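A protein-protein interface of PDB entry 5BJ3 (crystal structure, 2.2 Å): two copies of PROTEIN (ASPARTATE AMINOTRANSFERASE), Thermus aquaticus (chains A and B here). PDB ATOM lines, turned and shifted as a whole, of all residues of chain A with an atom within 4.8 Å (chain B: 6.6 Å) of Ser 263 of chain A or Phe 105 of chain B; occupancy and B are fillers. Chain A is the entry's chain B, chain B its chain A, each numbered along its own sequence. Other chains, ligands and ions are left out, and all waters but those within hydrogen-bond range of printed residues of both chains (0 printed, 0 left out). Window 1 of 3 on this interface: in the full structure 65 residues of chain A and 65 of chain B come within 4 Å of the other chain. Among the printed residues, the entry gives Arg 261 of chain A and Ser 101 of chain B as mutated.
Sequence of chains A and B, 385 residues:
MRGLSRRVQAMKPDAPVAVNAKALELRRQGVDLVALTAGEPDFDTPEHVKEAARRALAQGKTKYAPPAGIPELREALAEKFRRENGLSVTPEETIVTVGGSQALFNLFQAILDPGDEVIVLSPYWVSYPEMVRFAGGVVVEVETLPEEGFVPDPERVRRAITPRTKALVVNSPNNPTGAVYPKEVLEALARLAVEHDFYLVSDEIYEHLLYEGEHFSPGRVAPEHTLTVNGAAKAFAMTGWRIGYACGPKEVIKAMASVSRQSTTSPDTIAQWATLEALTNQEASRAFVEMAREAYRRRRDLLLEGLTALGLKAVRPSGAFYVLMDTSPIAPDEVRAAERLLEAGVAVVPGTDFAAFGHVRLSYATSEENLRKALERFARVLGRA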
ATOM      1  N   GLN A 102      -3.049  20.645   9.639  1.00  0.00           N
ATOM      2  CA  GLN A 102      -4.321  21.367   9.671  1.00  0.00           C
ATOM      3  C   GLN A 102      -5.253  20.795  10.735  1.00  0.00           C
ATOM      4  O   GLN A 102      -6.146  21.493  11.213  1.00  0.00           O
ATOM      5  CB  GLN A 102      -5.034  21.373   8.321  1.00  0.00           C
ATOM      6  CG  GLN A 102      -6.188  22.379   8.309  1.00  0.00           C
ATOM      7  CD  GLN A 102      -7.235  22.136   7.236  1.00  0.00           C
ATOM      8  OE1 GLN A 102      -7.822  23.078   6.708  1.00  0.00           O
ATOM      9  NE2 GLN A 102      -7.503  20.870   6.940  1.00  0.00           N
ATOM     10  N   PHE A 105      -4.071  22.626  13.729  1.00  0.00           N
ATOM     11  CA  PHE A 105      -4.441  24.034  13.586  1.00  0.00           C
ATOM     12  C   PHE A 105      -5.931  24.269  13.847  1.00  0.00           C
ATOM     13  O   PHE A 105      -6.298  25.158  14.618  1.00  0.00           O
ATOM     14  CB  PHE A 105      -4.067  24.542  12.186  1.00  0.00           C
ATOM     15  CG  PHE A 105      -4.396  25.994  11.955  1.00  0.00           C
ATOM     16  CD1 PHE A 105      -3.501  26.987  12.338  1.00  0.00           C
ATOM     17  CD2 PHE A 105      -5.601  26.367  11.368  1.00  0.00           C
ATOM     18  CE1 PHE A 105      -3.802  28.330  12.137  1.00  0.00           C
ATOM     19  CE2 PHE A 105      -5.910  27.711  11.162  1.00  0.00           C
ATOM     20  CZ  PHE A 105      -5.007  28.694  11.549  1.00  0.00           C
ATOM     21  N   VAL A 259     -14.373  24.849  10.846  1.00  0.00           N
ATOM     22  CA  VAL A 259     -13.220  25.684  10.535  1.00  0.00           C
ATOM     23  C   VAL A 259     -12.737  25.354   9.124  1.00  0.00           C
ATOM     24  O   VAL A 259     -12.331  26.241   8.381  1.00  0.00           O
ATOM     25  CB  VAL A 259     -12.072  25.479  11.547  1.00  0.00           C
ATOM     26  CG1 VAL A 259     -10.902  26.394  11.218  1.00  0.00           C
ATOM     27  CG2 VAL A 259     -12.563  25.750  12.959  1.00  0.00           C
ATOM     28  N   SER A 260     -12.810  24.079   8.749  1.00  0.00           N
ATOM     29  CA  SER A 260     -12.396  23.645   7.417  1.00  0.00           C
ATOM     30  C   SER A 260     -13.293  24.244   6.344  1.00  0.00           C
ATOM     31  O   SER A 260     -12.810  24.706   5.318  1.00  0.00           O
ATOM     32  CB  SER A 260     -12.425  22.120   7.310  1.00  0.00           C
ATOM     33  OG  SER A 260     -11.414  21.540   8.111  1.00  0.00           O
ATOM     34  N   ARG A 261     -14.597  24.255   6.606  1.00  0.00           N
ATOM     35  CA  ARG A 261     -15.579  24.794   5.676  1.00  0.00           C
ATOM     36  C   ARG A 261     -15.278  26.251   5.311  1.00  0.00           C
ATOM     37  O   ARG A 261     -15.432  26.652   4.158  1.00  0.00           O
ATOM     38  CB  ARG A 261     -16.982  24.688   6.282  1.00  0.00           C
ATOM     39  CG  ARG A 261     -18.117  24.945   5.304  1.00  0.00           C
ATOM     40  CD  ARG A 261     -19.463  24.976   6.015  1.00  0.00           C
ATOM     41  NE  ARG A 261     -19.590  26.131   6.906  1.00  0.00           N
ATOM     42  CZ  ARG A 261     -19.876  26.057   8.204  1.00  0.00           C
ATOM     43  NH1 ARG A 261     -20.075  24.878   8.783  1.00  0.00           N
ATOM     44  NH2 ARG A 261     -19.963  27.166   8.926  1.00  0.00           N
ATOM     45  N   GLN A 262     -14.817  27.025   6.295  1.00  0.00           N
ATOM     46  CA  GLN A 262     -14.498  28.434   6.084  1.00  0.00           C
ATOM     47  C   GLN A 262     -13.057  28.734   5.702  1.00  0.00           C
ATOM     48  O   GLN A 262     -12.670  29.898   5.604  1.00  0.00           O
ATOM     49  CB  GLN A 262     -14.859  29.254   7.324  1.00  0.00           C
ATOM     50  CG  GLN A 262     -16.339  29.250   7.657  1.00  0.00           C
ATOM     51  CD  GLN A 262     -17.236  29.589   6.472  1.00  0.00           C
ATOM     52  OE1 GLN A 262     -18.400  29.194   6.436  1.00  0.00           O
ATOM     53  NE2 GLN A 262     -16.700  30.334   5.507  1.00  0.00           N
ATOM     54  N   SER A 263     -12.255  27.698   5.491  1.00  0.00           N
ATOM     55  CA  SER A 263     -10.864  27.913   5.131  1.00  0.00           C
ATOM     56  C   SER A 263     -10.451  27.184   3.863  1.00  0.00           C
ATOM     57  O   SER A 263     -10.314  27.797   2.810  1.00  0.00           O
ATOM     58  CB  SER A 263      -9.944  27.534   6.296  1.00  0.00           C
ATOM     59  OG  SER A 263     -10.212  26.226   6.775  1.00  0.00           O
ATOM     60  N   THR A 264     -10.289  25.870   3.963  1.00  0.00           N
ATOM     61  CA  THR A 264      -9.870  25.051   2.834  1.00  0.00           C
ATOM     62  C   THR A 264     -11.025  24.391   2.086  1.00  0.00           C
ATOM     63  O   THR A 264     -10.836  23.884   0.981  1.00  0.00           O
ATOM     64  CB  THR A 264      -8.926  23.946   3.319  1.00  0.00           C
ATOM     65  OG1 THR A 264      -9.520  23.297   4.447  1.00  0.00           O
ATOM     66  CG2 THR A 264      -7.581  24.528   3.733  1.00  0.00           C
ATOM     67  N   THR A 265     -12.213  24.420   2.695  1.00  0.00           N
ATOM     68  CA  THR A 265     -13.439  23.813   2.160  1.00  0.00           C
ATOM     69  C   THR A 265     -13.417  22.299   2.396  1.00  0.00           C
ATOM     70  O   THR A 265     -14.312  21.755   3.042  1.00  0.00           O
ATOM     71  CB  THR A 265     -13.661  24.134   0.656  1.00  0.00           C
ATOM     72  OG1 THR A 265     -13.704  25.554   0.468  1.00  0.00           O
ATOM     73  CG2 THR A 265     -14.980  23.544   0.174  1.00  0.00           C
ATOM     74  N   VAL B  98      -4.617  26.523  -0.894  1.00  0.00           N
ATOM     75  CA  VAL B  98      -5.540  25.395  -0.996  1.00  0.00           C
ATOM     76  C   VAL B  98      -6.903  25.977  -1.354  1.00  0.00           C
ATOM     77  O   VAL B  98      -7.768  26.178  -0.495  1.00  0.00           O
ATOM     78  CB  VAL B  98      -5.609  24.581   0.328  1.00  0.00           C
ATOM     79  CG1 VAL B  98      -6.608  23.444   0.207  1.00  0.00           C
ATOM     80  CG2 VAL B  98      -4.237  24.016   0.668  1.00  0.00           C
ATOM     81  N   GLY B  99      -7.058  26.283  -2.636  1.00  0.00           N
ATOM     82  CA  GLY B  99      -8.286  26.868  -3.131  1.00  0.00           C
ATOM     83  C   GLY B  99      -8.273  28.371  -2.916  1.00  0.00           C
ATOM     84  O   GLY B  99      -7.461  28.891  -2.152  1.00  0.00           O
ATOM     85  N   GLY B 100      -9.146  29.078  -3.628  1.00  0.00           N
ATOM     86  CA  GLY B 100      -9.229  30.521  -3.472  1.00  0.00           C
ATOM     87  C   GLY B 100      -9.743  30.833  -2.082  1.00  0.00           C
ATOM     88  O   GLY B 100      -9.439  31.885  -1.524  1.00  0.00           O
ATOM     89  N   SER B 101     -10.498  29.896  -1.512  1.00  0.00           N
ATOM     90  CA  SER B 101     -11.054  30.055  -0.175  1.00  0.00           C
ATOM     91  C   SER B 101      -9.963  30.239   0.880  1.00  0.00           C
ATOM     92  O   SER B 101     -10.101  31.089   1.759  1.00  0.00           O
ATOM     93  CB  SER B 101     -11.964  28.872   0.178  1.00  0.00           C
ATOM     94  OG  SER B 101     -11.272  27.637   0.099  1.00  0.00           O
ATOM     95  N   GLN B 102      -8.878  29.466   0.795  1.00  0.00           N
ATOM     96  CA  GLN B 102      -7.799  29.614   1.770  1.00  0.00           C
ATOM     97  C   GLN B 102      -7.028  30.912   1.544  1.00  0.00           C
ATOM     98  O   GLN B 102      -6.409  31.439   2.467  1.00  0.00           O
ATOM     99  CB  GLN B 102      -6.824  28.434   1.765  1.00  0.00           C
ATOM    100  CG  GLN B 102      -5.912  28.464   3.000  1.00  0.00           C
ATOM    101  CD  GLN B 102      -4.633  27.665   2.867  1.00  0.00           C
ATOM    102  OE1 GLN B 102      -4.125  27.129   3.851  1.00  0.00           O
ATOM    103  NE2 GLN B 102      -4.073  27.625   1.668  1.00  0.00           N
ATOM    104  N   ALA B 103      -7.044  31.413   0.310  1.00  0.00           N
ATOM    105  CA  ALA B 103      -6.362  32.665   0.001  1.00  0.00           C
ATOM    106  C   ALA B 103      -7.086  33.770   0.767  1.00  0.00           C
ATOM    107  O   ALA B 103      -6.458  34.608   1.409  1.00  0.00           O
ATOM    108  CB  ALA B 103      -6.404  32.939  -1.496  1.00  0.00           C
ATOM    109  N   LEU B 104      -8.414  33.727   0.723  1.00  0.00           N
ATOM    110  CA  LEU B 104      -9.252  34.696   1.418  1.00  0.00           C
ATOM    111  C   LEU B 104      -9.114  34.550   2.933  1.00  0.00           C
ATOM    112  O   LEU B 104      -8.961  35.542   3.643  1.00  0.00           O
ATOM    113  CB  LEU B 104     -10.715  34.518   1.003  1.00  0.00           C
ATOM    114  CG  LEU B 104     -11.065  34.947  -0.424  1.00  0.00           C
ATOM    115  CD1 LEU B 104     -12.380  34.327  -0.857  1.00  0.00           C
ATOM    116  CD2 LEU B 104     -11.126  36.465  -0.506  1.00  0.00           C
ATOM    117  N   PHE B 105      -9.136  33.306   3.415  1.00  0.00           N
ATOM    118  CA  PHE B 105      -9.018  33.013   4.842  1.00  0.00           C
ATOM    119  C   PHE B 105      -7.693  33.505   5.420  1.00  0.00           C
ATOM    120  O   PHE B 105      -7.673  34.178   6.450  1.00  0.00           O
ATOM    121  CB  PHE B 105      -9.173  31.506   5.092  1.00  0.00           C
ATOM    122  CG  PHE B 105      -9.084  31.118   6.543  1.00  0.00           C
ATOM    123  CD1 PHE B 105     -10.211  31.171   7.358  1.00  0.00           C
ATOM    124  CD2 PHE B 105      -7.873  30.706   7.099  1.00  0.00           C
ATOM    125  CE1 PHE B 105     -10.134  30.819   8.706  1.00  0.00           C
ATOM    126  CE2 PHE B 105      -7.783  30.352   8.443  1.00  0.00           C
ATOM    127  CZ  PHE B 105      -8.919  30.411   9.249  1.00  0.00           C
ATOM    128  N   ASN B 106      -6.593  33.151   4.763  1.00  0.00           N
ATOM    129  CA  ASN B 106      -5.265  33.559   5.213  1.00  0.00           C
ATOM    130  C   ASN B 106      -5.115  35.072   5.180  1.00  0.00           C
ATOM    131  O   ASN B 106      -4.479  35.659   6.055  1.00  0.00           O
ATOM    132  CB  ASN B 106      -4.180  32.915   4.346  1.00  0.00           C
ATOM    133  CG  ASN B 106      -4.039  31.426   4.592  1.00  0.00           C
ATOM    134  OD1 ASN B 106      -4.863  30.812   5.273  1.00  0.00           O
ATOM    135  ND2 ASN B 106      -2.987  30.832   4.035  1.00  0.00           N
ATOM    136  N   LEU B 107      -5.718  35.693   4.167  1.00  0.00           N
ATOM    137  CA  LEU B 107      -5.671  37.141   3.999  1.00  0.00           C
ATOM    138  C   LEU B 107      -6.290  37.845   5.205  1.00  0.00           C
ATOM    139  O   LEU B 107      -5.663  38.700   5.814  1.00  0.00           O
ATOM    140  CB  LEU B 107      -6.403  37.535   2.710  1.00  0.00           C
ATOM    141  CG  LEU B 107      -6.345  38.964   2.162  1.00  0.00           C
ATOM    142  CD1 LEU B 107      -6.656  38.923   0.677  1.00  0.00           C
ATOM    143  CD2 LEU B 107      -7.326  39.873   2.874  1.00  0.00           C
ATOM    144  N   PHE B 108      -7.512  37.459   5.557  1.00  0.00           N
ATOM    145  CA  PHE B 108      -8.205  38.057   6.695  1.00  0.00           C
ATOM    146  C   PHE B 108      -7.510  37.788   8.026  1.00  0.00           C
ATOM    147  O   PHE B 108      -7.551  38.621   8.929  1.00  0.00           O
ATOM    148  CB  PHE B 108      -9.663  37.602   6.731  1.00  0.00           C
ATOM    149  CG  PHE B 108     -10.489  38.150   5.600  1.00  0.00           C
ATOM    150  CD1 PHE B 108     -10.454  39.511   5.296  1.00  0.00           C
ATOM    151  CD2 PHE B 108     -11.287  37.310   4.826  1.00  0.00           C
ATOM    152  CE1 PHE B 108     -11.200  40.025   4.237  1.00  0.00           C
ATOM    153  CE2 PHE B 108     -12.039  37.820   3.763  1.00  0.00           C
ATOM    154  CZ  PHE B 108     -11.994  39.177   3.470  1.00  0.00           C
ATOM    155  N   GLN B 109      -6.866  36.629   8.145  1.00  0.00           N
ATOM    156  CA  GLN B 109      -6.137  36.285   9.365  1.00  0.00           C
ATOM    157  C   GLN B 109      -4.862  37.126   9.445  1.00  0.00           C
ATOM    158  O   GLN B 109      -4.357  37.400  10.528  1.00  0.00           O
ATOM    159  CB  GLN B 109      -5.765  34.795   9.371  1.00  0.00           C
ATOM    160  CG  GLN B 109      -6.938  33.844   9.586  1.00  0.00           C
ATOM    161  CD  GLN B 109      -7.473  33.880  11.007  1.00  0.00           C
ATOM    162  OE1 GLN B 109      -6.706  33.883  11.967  1.00  0.00           O
ATOM    163  NE2 GLN B 109      -8.793  33.892  11.146  1.00  0.00           N
ATOM    164  N   ALA B 110      -4.361  37.542   8.287  1.00  0.00           N
ATOM    165  CA  ALA B 110      -3.139  38.333   8.198  1.00  0.00           C
ATOM    166  C   ALA B 110      -3.312  39.850   8.302  1.00  0.00           C
ATOM    167  O   ALA B 110      -2.350  40.551   8.608  1.00  0.00           O
ATOM    168  CB  ALA B 110      -2.390  37.982   6.915  1.00  0.00           C
ATOM    169  N   MET B 131     -15.646  34.308   7.224  1.00  0.00           N
ATOM    170  CA  MET B 131     -14.203  34.464   7.323  1.00  0.00           C
ATOM    171  C   MET B 131     -13.809  35.743   8.046  1.00  0.00           C
ATOM    172  O   MET B 131     -12.840  35.762   8.807  1.00  0.00           O
ATOM    173  CB  MET B 131     -13.579  34.464   5.930  1.00  0.00           C
ATOM    174  CG  MET B 131     -13.742  33.172   5.158  1.00  0.00           C
ATOM    175  SD  MET B 131     -13.170  33.393   3.468  1.00  0.00           S
ATOM    176  CE  MET B 131     -13.477  31.799   2.784  1.00  0.00           C
ATOM    177  N   PHE B 134     -14.556  35.334  11.842  1.00  0.00           N
ATOM    178  CA  PHE B 134     -13.665  34.345  12.436  1.00  0.00           C
ATOM    179  C   PHE B 134     -12.325  34.968  12.828  1.00  0.00           C
ATOM    180  O   PHE B 134     -11.656  34.481  13.737  1.00  0.00           O
ATOM    181  CB  PHE B 134     -13.446  33.175  11.470  1.00  0.00           C
ATOM    182  CG  PHE B 134     -12.991  31.912  12.148  1.00  0.00           C
ATOM    183  CD1 PHE B 134     -13.891  31.131  12.869  1.00  0.00           C
ATOM    184  CD2 PHE B 134     -11.662  31.501  12.073  1.00  0.00           C
ATOM    185  CE1 PHE B 134     -13.479  29.969  13.509  1.00  0.00           C
ATOM    186  CE2 PHE B 134     -11.240  30.336  12.709  1.00  0.00           C
ATOM    187  CZ  PHE B 134     -12.150  29.569  13.428  1.00  0.00           C
ATOM    188  N   ALA B 135     -11.946  36.045  12.143  1.00  0.00           N
ATOM    189  CA  ALA B 135     -10.693  36.744  12.429  1.00  0.00           C
ATOM    190  C   ALA B 135     -10.901  37.892  13.421  1.00  0.00           C
ATOM    191  O   ALA B 135      -9.950  38.571  13.807  1.00  0.00           O
ATOM    192  CB  ALA B 135     -10.069  37.265  11.137  1.00  0.00           C
ATOM    193  N   ARG B 242      -8.371  21.730  -5.305  1.00  0.00           N
ATOM    194  CA  ARG B 242      -8.036  22.660  -4.233  1.00  0.00           C
ATOM    195  C   ARG B 242      -6.764  23.489  -4.443  1.00  0.00           C
ATOM    196  O   ARG B 242      -5.853  23.459  -3.615  1.00  0.00           O
ATOM    197  CB  ARG B 242      -7.951  21.907  -2.901  1.00  0.00           C
ATOM    198  CG  ARG B 242      -9.209  21.138  -2.514  1.00  0.00           C
ATOM    199  CD  ARG B 242     -10.259  22.040  -1.893  1.00  0.00           C
ATOM    200  NE  ARG B 242     -10.913  22.875  -2.879  1.00  0.00           N
ATOM    201  CZ  ARG B 242     -11.205  24.158  -2.707  1.00  0.00           C
ATOM    202  NH1 ARG B 242     -10.908  24.792  -1.582  1.00  0.00           N
ATOM    203  NH2 ARG B 242     -11.798  24.806  -3.686  1.00  0.00           N
ATOM    204  N   VAL B 259       0.928  32.062   7.458  1.00  0.00           N
ATOM    205  CA  VAL B 259      -0.266  31.415   7.986  1.00  0.00           C
ATOM    206  C   VAL B 259      -0.369  30.006   7.398  1.00  0.00           C
ATOM    207  O   VAL B 259      -0.768  29.070   8.083  1.00  0.00           O
ATOM    208  CB  VAL B 259      -1.548  32.220   7.654  1.00  0.00           C
ATOM    209  CG1 VAL B 259      -2.771  31.539   8.248  1.00  0.00           C
ATOM    210  CG2 VAL B 259      -1.427  33.639   8.192  1.00  0.00           C
ATOM    211  N   SER B 263      -0.493  26.031   9.142  1.00  0.00           N
ATOM    212  CA  SER B 263      -1.790  25.392   9.006  1.00  0.00           C
ATOM    213  C   SER B 263      -1.780  24.200   8.061  1.00  0.00           C
ATOM    214  O   SER B 263      -1.807  23.053   8.503  1.00  0.00           O
ATOM    215  CB  SER B 263      -2.846  26.416   8.579  1.00  0.00           C
ATOM    216  OG  SER B 263      -2.433  27.141   7.433  1.00  0.00           O
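Of the 19 printed residues of chain B, 8 touch a printed residue of chain A. Hydrophobic or aromatic side chains of chain B that line the printed part of chain A: Val 98, Phe 105, Met 131 and Phe 134. Among the printed residues, no Asp or Glu carboxylate lies within 4 Å of a Lys or Arg side-chain nitrogen of the other chain.
Gln 102 of chain A touches Ser 263 of chain B, and with the chains exchanged Ser 263 of chain A touches Gln 102 of chain B. Phe 105 of chain A touches Ser 263 of chain B, and with the chains exchanged Ser 263 of chain A touches Phe 105 of chain B. Of the 13 pairs that touch across the chains among the printed residues, 4 have their exchanged pair printed and touching as well.
Phe 105 of chain A touches Ser 263 of chain B (CG to CB, 3.7 Å). CG2 of Val 259 of chain A touches CZ of Phe 134 of chain B, at 3.9 Å. Phe 105 of chain B touches Gln 262 of chain A. Gln 262 of chain A touches Met 131 of chain B. CB of Ser 263 of chain A touches CG of Phe 105 of chain B, 3.7 Å away. Thr 264 of chain A touches Val 98 of chain B (CG2 to CG1, 3.8 Å). Thr 264 of chain A touches Ser 101 of chain B. OG1 of Thr 265 of chain A touches NH1 of Arg 242 of chain B (3.5 Å).
The backbone carbonyl oxygen (O) of Ser 260 of chain A is in hydrogen-bond range of the side-chain hydroxyl (OG) of Ser 263 of chain A, at 3.3 Å. The side-chain amide oxygen of Gln 102 of chain A is in hydrogen-bond range of the side-chain hydroxyl of Thr 264 of chain A, at 2.8 Å. OG of Ser 101 of chain B is in hydrogen-bond range of NH1 of Arg 242 of chain B, 3.3 Å away. The backbone carbonyl oxygen (O) of Val 259 of chain A sits at hydrogen-bond distance from the side-chain hydroxyl (OG) of Ser 263 of chain A (2.7 Å). O of Gln 102 of chain B lies close to OD1 of Asn 106 of chain B (3.3 Å). The backbone carbonyl oxygen of Ser 260 of chain A lies within hydrogen-bond range of the backbone NH of Thr 265 of chain A (2.7 Å).
O of Ser 263 of chain A lies within hydrogen-bond range of OG of Ser 101 of chain B (2.9 Å). The guanidinium group (NH1) of Arg 242 of chain B sits at hydrogen-bond distance from the backbone carbonyl oxygen (O) of Thr 264 of chain A (2.7 Å). The backbone NH (N) of Gln 102 of chain B lies within hydrogen-bond range of the backbone carbonyl oxygen (O) of Ser 263 of chain A, 3.0 Å away. The side-chain hydroxyl of Ser 101 of chain B lies within hydrogen-bond range of the side-chain hydroxyl of Thr 265 of chain A, at 3.2 Å. The backbone carbonyl oxygen of Ser 263 of chain B lies within hydrogen-bond range of the backbone NH of Gln 102 of chain A (2.9 Å).
Of the printed residues of chain B, Gln 102 of chain A touches Ser 263. Of the printed residues of chain B, Phe 105 of chain A touches Ser 263. Of the printed residues of chain B, Gln 262 of chain A touches Phe 105 (3.3 Å) and Met 131 (3.5 Å). Of chain B, only Ser 101 (2.9 Å), Gln 102 (3.0 Å) and Phe 105 (3.7 Å) come within 4 Å of Ser 263 of chain A. Of the printed residues of chain A, Gln 102 of chain B touches Ser 263 (3.0 Å). Of chain A, only Gln 262 and Ser 263 come within 4 Å of Phe 105 of chain B. Phe 108 of chain B touches none of the printed residues of chain A. Of the printed residues of chain A, Ser 263 of chain B touches Gln 102 (2.9 Å) and Phe 105 (3.7 Å). The nearest residue of chain B that does not touch Ser 263 of chain A is Val 98 of chain B (4.5 Å). The nearest printed residue of chain A that does not touch Gln 102 of chain B is Thr 264 of chain A (4.3 Å).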
